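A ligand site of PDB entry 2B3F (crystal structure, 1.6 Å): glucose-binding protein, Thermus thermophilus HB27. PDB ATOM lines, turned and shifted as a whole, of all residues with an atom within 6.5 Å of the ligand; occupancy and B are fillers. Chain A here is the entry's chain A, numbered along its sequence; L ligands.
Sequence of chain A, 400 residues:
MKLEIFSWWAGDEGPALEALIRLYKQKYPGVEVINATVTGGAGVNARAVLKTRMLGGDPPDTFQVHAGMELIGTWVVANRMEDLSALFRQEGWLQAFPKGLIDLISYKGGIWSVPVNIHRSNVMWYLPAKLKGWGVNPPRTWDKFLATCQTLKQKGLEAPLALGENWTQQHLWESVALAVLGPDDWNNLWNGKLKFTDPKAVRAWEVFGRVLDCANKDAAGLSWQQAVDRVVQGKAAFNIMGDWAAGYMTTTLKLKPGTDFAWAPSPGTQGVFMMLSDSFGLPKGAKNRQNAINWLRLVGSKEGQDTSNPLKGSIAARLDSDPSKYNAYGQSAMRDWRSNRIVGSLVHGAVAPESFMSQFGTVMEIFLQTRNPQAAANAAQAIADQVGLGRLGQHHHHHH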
ATOM      1  N   TRP A   8       8.503  22.347  14.998  1.00  0.00           N
ATOM      2  CA  TRP A   8       7.769  23.621  15.023  1.00  0.00           C
ATOM      3  C   TRP A   8       8.135  24.492  16.211  1.00  0.00           C
ATOM      4  O   TRP A   8       7.364  25.382  16.628  1.00  0.00           O
ATOM      5  CB  TRP A   8       6.262  23.384  14.893  1.00  0.00           C
ATOM      6  CG  TRP A   8       5.541  22.630  15.926  1.00  0.00           C
ATOM      7  CD1 TRP A   8       4.912  23.128  17.038  1.00  0.00           C
ATOM      8  CD2 TRP A   8       5.225  21.231  15.887  1.00  0.00           C
ATOM      9  NE1 TRP A   8       4.239  22.121  17.718  1.00  0.00           N
ATOM     10  CE2 TRP A   8       4.418  20.948  17.019  1.00  0.00           C
ATOM     11  CE3 TRP A   8       5.554  20.198  15.012  1.00  0.00           C
ATOM     12  CZ2 TRP A   8       3.946  19.660  17.290  1.00  0.00           C
ATOM     13  CZ3 TRP A   8       5.095  18.930  15.289  1.00  0.00           C
ATOM     14  CH2 TRP A   8       4.301  18.673  16.405  1.00  0.00           C
ATOM     15  N   TRP A   9       9.352  24.293  16.738  1.00  0.00           N
ATOM     16  CA  TRP A   9       9.744  25.030  17.899  1.00  0.00           C
ATOM     17  C   TRP A   9      10.437  26.356  17.527  1.00  0.00           C
ATOM     18  O   TRP A   9      11.585  26.609  17.826  1.00  0.00           O
ATOM     19  CB  TRP A   9      10.594  24.132  18.797  1.00  0.00           C
ATOM     20  CG  TRP A   9       9.797  23.065  19.455  1.00  0.00           C
ATOM     21  CD1 TRP A   9       8.481  23.124  19.867  1.00  0.00           C
ATOM     22  CD2 TRP A   9      10.262  21.751  19.785  1.00  0.00           C
ATOM     23  NE1 TRP A   9       8.121  21.918  20.437  1.00  0.00           N
ATOM     24  CE2 TRP A   9       9.199  21.070  20.401  1.00  0.00           C
ATOM     25  CE3 TRP A   9      11.494  21.101  19.628  1.00  0.00           C
ATOM     26  CZ2 TRP A   9       9.322  19.767  20.870  1.00  0.00           C
ATOM     27  CZ3 TRP A   9      11.603  19.786  20.071  1.00  0.00           C
ATOM     28  CH2 TRP A   9      10.538  19.148  20.700  1.00  0.00           C
ATOM     29  N   GLU A  13       9.120  29.385  21.314  1.00  0.00           N
ATOM     30  CA  GLU A  13       9.115  27.951  21.616  1.00  0.00           C
ATOM     31  C   GLU A  13      10.499  27.323  21.528  1.00  0.00           C
ATOM     32  O   GLU A  13      10.669  26.153  21.932  1.00  0.00           O
ATOM     33  CB  GLU A  13       8.135  27.213  20.704  1.00  0.00           C
ATOM     34  CG  GLU A  13       6.671  27.672  20.889  1.00  0.00           C
ATOM     35  CD  GLU A  13       5.673  26.560  20.666  1.00  0.00           C
ATOM     36  OE1 GLU A  13       4.673  26.779  19.925  1.00  0.00           O
ATOM     37  OE2 GLU A  13       5.865  25.482  21.264  1.00  0.00           O
ATOM     38  N   GLY A  40       4.323  27.645  13.500  1.00  0.00           N
ATOM     39  CA  GLY A  40       2.889  27.388  13.641  1.00  0.00           C
ATOM     40  C   GLY A  40       2.591  26.510  14.842  1.00  0.00           C
ATOM     41  O   GLY A  40       3.121  25.398  14.967  1.00  0.00           O
ATOM     42  N   GLY A  41       1.759  27.015  15.732  1.00  0.00           N
ATOM     43  CA  GLY A  41       1.375  26.295  16.936  1.00  0.00           C
ATOM     44  C   GLY A  41       0.846  24.918  16.647  1.00  0.00           C
ATOM     45  O   GLY A  41       0.137  24.698  15.643  1.00  0.00           O
ATOM     46  N   ALA A  42       1.197  23.963  17.517  1.00  0.00           N
ATOM     47  CA  ALA A  42       0.671  22.597  17.469  1.00  0.00           C
ATOM     48  C   ALA A  42       0.985  21.827  16.183  1.00  0.00           C
ATOM     49  O   ALA A  42       0.390  20.777  15.918  1.00  0.00           O
ATOM     50  CB  ALA A  42      -0.858  22.554  17.733  1.00  0.00           C
ATOM     51  N   GLY A  43       1.939  22.311  15.406  1.00  0.00           N
ATOM     52  CA  GLY A  43       2.420  21.555  14.253  1.00  0.00           C
ATOM     53  C   GLY A  43       1.502  21.475  13.051  1.00  0.00           C
ATOM     54  O   GLY A  43       1.749  20.711  12.134  1.00  0.00           O
ATOM     55  N   ARG A  47       3.197  19.881   9.801  1.00  0.00           N
ATOM     56  CA  ARG A  47       2.585  18.654   9.224  1.00  0.00           C
ATOM     57  C   ARG A  47       2.505  18.782   7.692  1.00  0.00           C
ATOM     58  O   ARG A  47       2.907  17.872   6.949  1.00  0.00           O
ATOM     59  CB  ARG A  47       1.189  18.529   9.869  1.00  0.00           C
ATOM     60  CG  ARG A  47       0.361  17.267   9.776  1.00  0.00           C
ATOM     61  CD  ARG A  47      -0.699  17.284  10.938  1.00  0.00           C
ATOM     62  NE  ARG A  47      -0.027  17.101  12.250  1.00  0.00           N
ATOM     63  CZ  ARG A  47      -0.285  17.735  13.400  1.00  0.00           C
ATOM     64  NH1 ARG A  47      -1.242  18.654  13.507  1.00  0.00           N
ATOM     65  NH2 ARG A  47       0.460  17.457  14.466  1.00  0.00           N
ATOM     66  N   GLN A  64      10.247  16.345  14.539  1.00  0.00           N
ATOM     67  CA  GLN A  64       9.364  16.333  15.685  1.00  0.00           C
ATOM     68  C   GLN A  64       8.046  15.646  15.316  1.00  0.00           C
ATOM     69  O   GLN A  64       7.411  15.944  14.303  1.00  0.00           O
ATOM     70  CB  GLN A  64       9.081  17.762  16.123  1.00  0.00           C
ATOM     71  CG  GLN A  64       8.215  17.879  17.334  1.00  0.00           C
ATOM     72  CD  GLN A  64       7.812  19.335  17.641  1.00  0.00           C
ATOM     73  OE1 GLN A  64       8.315  20.264  17.015  1.00  0.00           O
ATOM     74  NE2 GLN A  64       6.924  19.516  18.610  1.00  0.00           N
ATOM     75  N   HIS A  66       4.543  13.477  17.290  1.00  0.00           N
ATOM     76  CA  HIS A  66       3.860  13.055  18.479  1.00  0.00           C
ATOM     77  C   HIS A  66       3.807  11.543  18.624  1.00  0.00           C
ATOM     78  O   HIS A  66       3.413  10.840  17.711  1.00  0.00           O
ATOM     79  CB  HIS A  66       2.436  13.594  18.509  1.00  0.00           C
ATOM     80  CG  HIS A  66       2.358  15.067  18.783  1.00  0.00           C
ATOM     81  ND1 HIS A  66       1.642  15.920  17.988  1.00  0.00           N
ATOM     82  CD2 HIS A  66       2.918  15.819  19.750  1.00  0.00           C
ATOM     83  CE1 HIS A  66       1.748  17.151  18.472  1.00  0.00           C
ATOM     84  NE2 HIS A  66       2.503  17.116  19.544  1.00  0.00           N
ATOM     85  N   ASN A 117       9.971  14.161  26.007  1.00  0.00           N
ATOM     86  CA  ASN A 117       9.240  14.815  27.054  1.00  0.00           C
ATOM     87  C   ASN A 117       7.855  14.202  27.265  1.00  0.00           C
ATOM     88  O   ASN A 117       7.441  13.254  26.575  1.00  0.00           O
ATOM     89  CB  ASN A 117       9.105  16.328  26.749  1.00  0.00           C
ATOM     90  CG  ASN A 117       8.226  16.613  25.533  1.00  0.00           C
ATOM     91  OD1 ASN A 117       7.601  15.727  24.982  1.00  0.00           O
ATOM     92  ND2 ASN A 117       8.183  17.884  25.120  1.00  0.00           N
ATOM     93  N   HIS A 119       4.206  16.378  27.824  1.00  0.00           N
ATOM     94  CA  HIS A 119       3.386  17.548  28.102  1.00  0.00           C
ATOM     95  C   HIS A 119       1.994  17.106  28.579  1.00  0.00           C
ATOM     96  O   HIS A 119       1.508  16.001  28.270  1.00  0.00           O
ATOM     97  CB  HIS A 119       3.206  18.450  26.854  1.00  0.00           C
ATOM     98  CG  HIS A 119       4.290  19.470  26.631  1.00  0.00           C
ATOM     99  ND1 HIS A 119       4.523  20.526  27.478  1.00  0.00           N
ATOM    100  CD2 HIS A 119       5.137  19.636  25.584  1.00  0.00           C
ATOM    101  CE1 HIS A 119       5.487  21.287  26.969  1.00  0.00           C
ATOM    102  NE2 HIS A 119       5.875  20.769  25.824  1.00  0.00           N
ATOM    103  N   TRP A 167      -6.855  25.642  16.382  1.00  0.00           N
ATOM    104  CA  TRP A 167      -6.345  24.478  17.150  1.00  0.00           C
ATOM    105  C   TRP A 167      -6.523  24.656  18.648  1.00  0.00           C
ATOM    106  O   TRP A 167      -6.730  23.676  19.367  1.00  0.00           O
ATOM    107  CB  TRP A 167      -4.917  24.094  16.774  1.00  0.00           C
ATOM    108  CG  TRP A 167      -3.863  24.926  17.327  1.00  0.00           C
ATOM    109  CD1 TRP A 167      -3.204  25.931  16.713  1.00  0.00           C
ATOM    110  CD2 TRP A 167      -3.283  24.808  18.639  1.00  0.00           C
ATOM    111  NE1 TRP A 167      -2.262  26.485  17.549  1.00  0.00           N
ATOM    112  CE2 TRP A 167      -2.285  25.799  18.738  1.00  0.00           C
ATOM    113  CE3 TRP A 167      -3.515  23.964  19.726  1.00  0.00           C
ATOM    114  CZ2 TRP A 167      -1.510  25.965  19.887  1.00  0.00           C
ATOM    115  CZ3 TRP A 167      -2.759  24.140  20.869  1.00  0.00           C
ATOM    116  CH2 TRP A 167      -1.764  25.131  20.940  1.00  0.00           C
ATOM    117  N   TRP A 224      -1.457  30.902  20.453  1.00  0.00           N
ATOM    118  CA  TRP A 224      -1.602  30.430  21.818  1.00  0.00           C
ATOM    119  C   TRP A 224      -0.883  31.335  22.800  1.00  0.00           C
ATOM    120  O   TRP A 224      -1.417  31.565  23.875  1.00  0.00           O
ATOM    121  CB  TRP A 224      -1.179  28.963  21.964  1.00  0.00           C
ATOM    122  CG  TRP A 224       0.298  28.688  21.921  1.00  0.00           C
ATOM    123  CD1 TRP A 224       1.036  28.269  20.860  1.00  0.00           C
ATOM    124  CD2 TRP A 224       1.219  28.771  23.030  1.00  0.00           C
ATOM    125  NE1 TRP A 224       2.351  28.074  21.221  1.00  0.00           N
ATOM    126  CE2 TRP A 224       2.487  28.408  22.540  1.00  0.00           C
ATOM    127  CE3 TRP A 224       1.088  29.142  24.367  1.00  0.00           C
ATOM    128  CZ2 TRP A 224       3.621  28.401  23.361  1.00  0.00           C
ATOM    129  CZ3 TRP A 224       2.223  29.161  25.159  1.00  0.00           C
ATOM    130  CH2 TRP A 224       3.456  28.775  24.659  1.00  0.00           C
ATOM    131  N   MET A 241      -4.717  25.415  28.335  1.00  0.00           N
ATOM    132  CA  MET A 241      -3.649  25.212  27.370  1.00  0.00           C
ATOM    133  C   MET A 241      -2.607  24.240  27.938  1.00  0.00           C
ATOM    134  O   MET A 241      -2.471  24.125  29.172  1.00  0.00           O
ATOM    135  CB  MET A 241      -3.019  26.565  27.032  1.00  0.00           C
ATOM    136  CG  MET A 241      -1.921  26.590  25.992  1.00  0.00           C
ATOM    137  SD  MET A 241      -2.341  25.691  24.490  1.00  0.00           S
ATOM    138  CE  MET A 241      -3.910  26.400  23.975  1.00  0.00           C
ATOM    139  N   TRP A 244       3.342  23.831  27.846  1.00  0.00           N
ATOM    140  CA  TRP A 244       4.270  24.731  27.137  1.00  0.00           C
ATOM    141  C   TRP A 244       3.991  26.187  27.574  1.00  0.00           C
ATOM    142  O   TRP A 244       4.857  27.047  27.476  1.00  0.00           O
ATOM    143  CB  TRP A 244       4.157  24.598  25.610  1.00  0.00           C
ATOM    144  CG  TRP A 244       2.772  24.537  25.050  1.00  0.00           C
ATOM    145  CD1 TRP A 244       1.994  25.572  24.582  1.00  0.00           C
ATOM    146  CD2 TRP A 244       2.012  23.329  24.821  1.00  0.00           C
ATOM    147  NE1 TRP A 244       0.790  25.077  24.111  1.00  0.00           N
ATOM    148  CE2 TRP A 244       0.773  23.717  24.262  1.00  0.00           C
ATOM    149  CE3 TRP A 244       2.250  21.976  25.075  1.00  0.00           C
ATOM    150  CZ2 TRP A 244      -0.208  22.777  23.925  1.00  0.00           C
ATOM    151  CZ3 TRP A 244       1.274  21.057  24.744  1.00  0.00           C
ATOM    152  CH2 TRP A 244       0.064  21.447  24.175  1.00  0.00           C
ATOM    153  N   LEU A 276       0.617  14.087  26.135  1.00  0.00           N
ATOM    154  CA  LEU A 276       1.157  13.980  24.792  1.00  0.00           C
ATOM    155  C   LEU A 276       2.677  13.908  24.951  1.00  0.00           C
ATOM    156  O   LEU A 276       3.196  14.227  26.035  1.00  0.00           O
ATOM    157  CB  LEU A 276       0.772  15.213  23.931  1.00  0.00           C
ATOM    158  CG  LEU A 276       1.192  16.557  24.523  1.00  0.00           C
ATOM    159  CD1 LEU A 276       2.040  17.365  23.562  1.00  0.00           C
ATOM    160  CD2 LEU A 276       0.014  17.361  25.096  1.00  0.00           C
ATOM    161  N   SER A 277       3.370  13.524  23.893  1.00  0.00           N
ATOM    162  CA  SER A 277       4.824  13.409  23.968  1.00  0.00           C
ATOM    163  C   SER A 277       5.442  13.764  22.645  1.00  0.00           C
ATOM    164  O   SER A 277       5.081  13.200  21.618  1.00  0.00           O
ATOM    165  CB  SER A 277       5.230  11.994  24.392  1.00  0.00           C
ATOM    166  OG  SER A 277       6.644  11.874  24.378  1.00  0.00           O
ATOM    167  N   ASP A 278       6.358  14.736  22.668  1.00  0.00           N
ATOM    168  CA  ASP A 278       7.175  15.082  21.539  1.00  0.00           C
ATOM    169  C   ASP A 278       8.286  14.045  21.427  1.00  0.00           C
ATOM    170  O   ASP A 278       8.903  13.706  22.430  1.00  0.00           O
ATOM    171  CB  ASP A 278       7.768  16.472  21.722  1.00  0.00           C
ATOM    172  CG  ASP A 278       6.689  17.578  21.722  1.00  0.00           C
ATOM    173  OD1 ASP A 278       5.907  17.586  20.746  1.00  0.00           O
ATOM    174  OD2 ASP A 278       6.655  18.381  22.674  1.00  0.00           O
ATOM    175  N   LYS A 312      11.243  24.222  28.725  1.00  0.00           N
ATOM    176  CA  LYS A 312      10.066  23.984  27.866  1.00  0.00           C
ATOM    177  C   LYS A 312       8.718  24.048  28.579  1.00  0.00           C
ATOM    178  O   LYS A 312       7.724  24.422  27.954  1.00  0.00           O
ATOM    179  CB  LYS A 312      10.206  22.604  27.220  1.00  0.00           C
ATOM    180  CG  LYS A 312       9.214  22.275  26.112  1.00  0.00           C
ATOM    181  CD  LYS A 312       9.433  23.018  24.838  1.00  0.00           C
ATOM    182  CE  LYS A 312       8.686  22.339  23.695  1.00  0.00           C
ATOM    183  NZ  LYS A 312       7.215  22.364  23.931  1.00  0.00           N
ATOM    184  N   VAL A 347      -5.685  16.459  20.116  1.00  0.00           N
ATOM    185  CA  VAL A 347      -5.141  17.546  19.325  1.00  0.00           C
ATOM    186  C   VAL A 347      -3.625  17.395  19.153  1.00  0.00           C
ATOM    187  O   VAL A 347      -3.041  17.850  18.165  1.00  0.00           O
ATOM    188  CB  VAL A 347      -5.530  18.901  19.960  1.00  0.00           C
ATOM    189  CG1 VAL A 347      -4.921  20.057  19.197  1.00  0.00           C
ATOM    190  CG2 VAL A 347      -7.058  18.998  20.000  1.00  0.00           C
ATOM    191  N   HIS A 348      -3.012  16.689  20.103  1.00  0.00           N
ATOM    192  CA  HIS A 348      -1.561  16.528  20.123  1.00  0.00           C
ATOM    193  C   HIS A 348      -1.133  15.058  19.900  1.00  0.00           C
ATOM    194  O   HIS A 348      -0.098  14.635  20.402  1.00  0.00           O
ATOM    195  CB  HIS A 348      -1.005  17.157  21.385  1.00  0.00           C
ATOM    196  CG  HIS A 348      -1.435  18.589  21.546  1.00  0.00           C
ATOM    197  ND1 HIS A 348      -0.877  19.605  20.813  1.00  0.00           N
ATOM    198  CD2 HIS A 348      -2.428  19.127  22.280  1.00  0.00           C
ATOM    199  CE1 HIS A 348      -1.509  20.731  21.102  1.00  0.00           C
ATOM    200  NE2 HIS A 348      -2.457  20.473  21.992  1.00  0.00           N
HETATM  201  C1  LIG L   1       2.258  20.703  20.728  1.00  0.00           C
HETATM  202  C2  LIG L   1       3.708  20.249  20.928  1.00  0.00           C
HETATM  203  C3  LIG L   1       4.434  21.120  21.945  1.00  0.00           C
HETATM  204  C4  LIG L   1       4.301  22.602  21.599  1.00  0.00           C
HETATM  205  C5  LIG L   1       2.809  22.907  21.316  1.00  0.00           C
HETATM  206  C6  LIG L   1       2.506  24.365  20.938  1.00  0.00           C
HETATM  207  O1  LIG L   1       1.624  19.941  19.748  1.00  0.00           O
HETATM  208  O2  LIG L   1       3.718  18.861  21.311  1.00  0.00           O
HETATM  209  O3  LIG L   1       5.815  20.770  21.978  1.00  0.00           O
HETATM  210  O4  LIG L   1       5.126  22.855  20.494  1.00  0.00           O
HETATM  211  O5  LIG L   1       2.283  22.070  20.313  1.00  0.00           O
HETATM  212  O6  LIG L   1       2.973  24.646  19.661  1.00  0.00           O
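A ring nitrogen (NE2) of His 66 is in hydrogen-bond range of an oxygen (O2) of the ligand (2.8 Å). The indole nitrogen (NE1) of Trp 8 is in hydrogen-bond range of an oxygen (O4) of the ligand. An oxygen (O6) of the ligand sits at hydrogen-bond distance from the side-chain carboxylate of Glu 13 (2.7 Å). O1 of the ligand lies within hydrogen-bond range of ND1 of His 348. The side-chain carboxylate (OD1) of Asp 278 lies within hydrogen-bond range of an oxygen (O2) of the ligand, 2.6 Å away. NZ of Lys 312 sits at hydrogen-bond distance from O3 of the ligand (2.9 Å). The indole nitrogen (NE1) of Trp 9 lies within hydrogen-bond range of an oxygen (O3) of the ligand, 3.0 Å away. An oxygen (O6) of the ligand is in hydrogen-bond range of the backbone NH of Ala 42.
Merely in contact with the ligand: Leu 276, Gly 41, Trp 244, Trp 224, Gln 64 and His 119.
The backbone NH (N) of Asp 278 lies within hydrogen-bond range of the side-chain amide oxygen (OD1) of Asn 117 (2.8 Å). The indole nitrogen (NE1) of Trp 244 is in hydrogen-bond range of the side-chain sulfur (SD) of Met 241 (3.2 Å). OD1 of Asp 278 is in hydrogen-bond range of NE2 of Gln 64, at 3.1 Å. The side-chain amino group (NZ) of Lys 312 is in hydrogen-bond range of a ring nitrogen (NE2) of His 119 (2.8 Å). The indole nitrogen (NE1) of Trp 224 lies within hydrogen-bond range of the side-chain carboxylate (OE1) of Glu 13, at 3.0 Å. The side-chain amide oxygen (OE1) of Gln 64 sits at hydrogen-bond distance from the backbone NH (N) of Trp 8 (2.9 Å). The indole nitrogen (NE1) of Trp 9 lies close to the side-chain amide nitrogen (NE2) of Gln 64, at 3.2 Å. The backbone carbonyl oxygen (O) of His 348 sits close to a ring nitrogen (ND1) of His 66 (3.2 Å).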
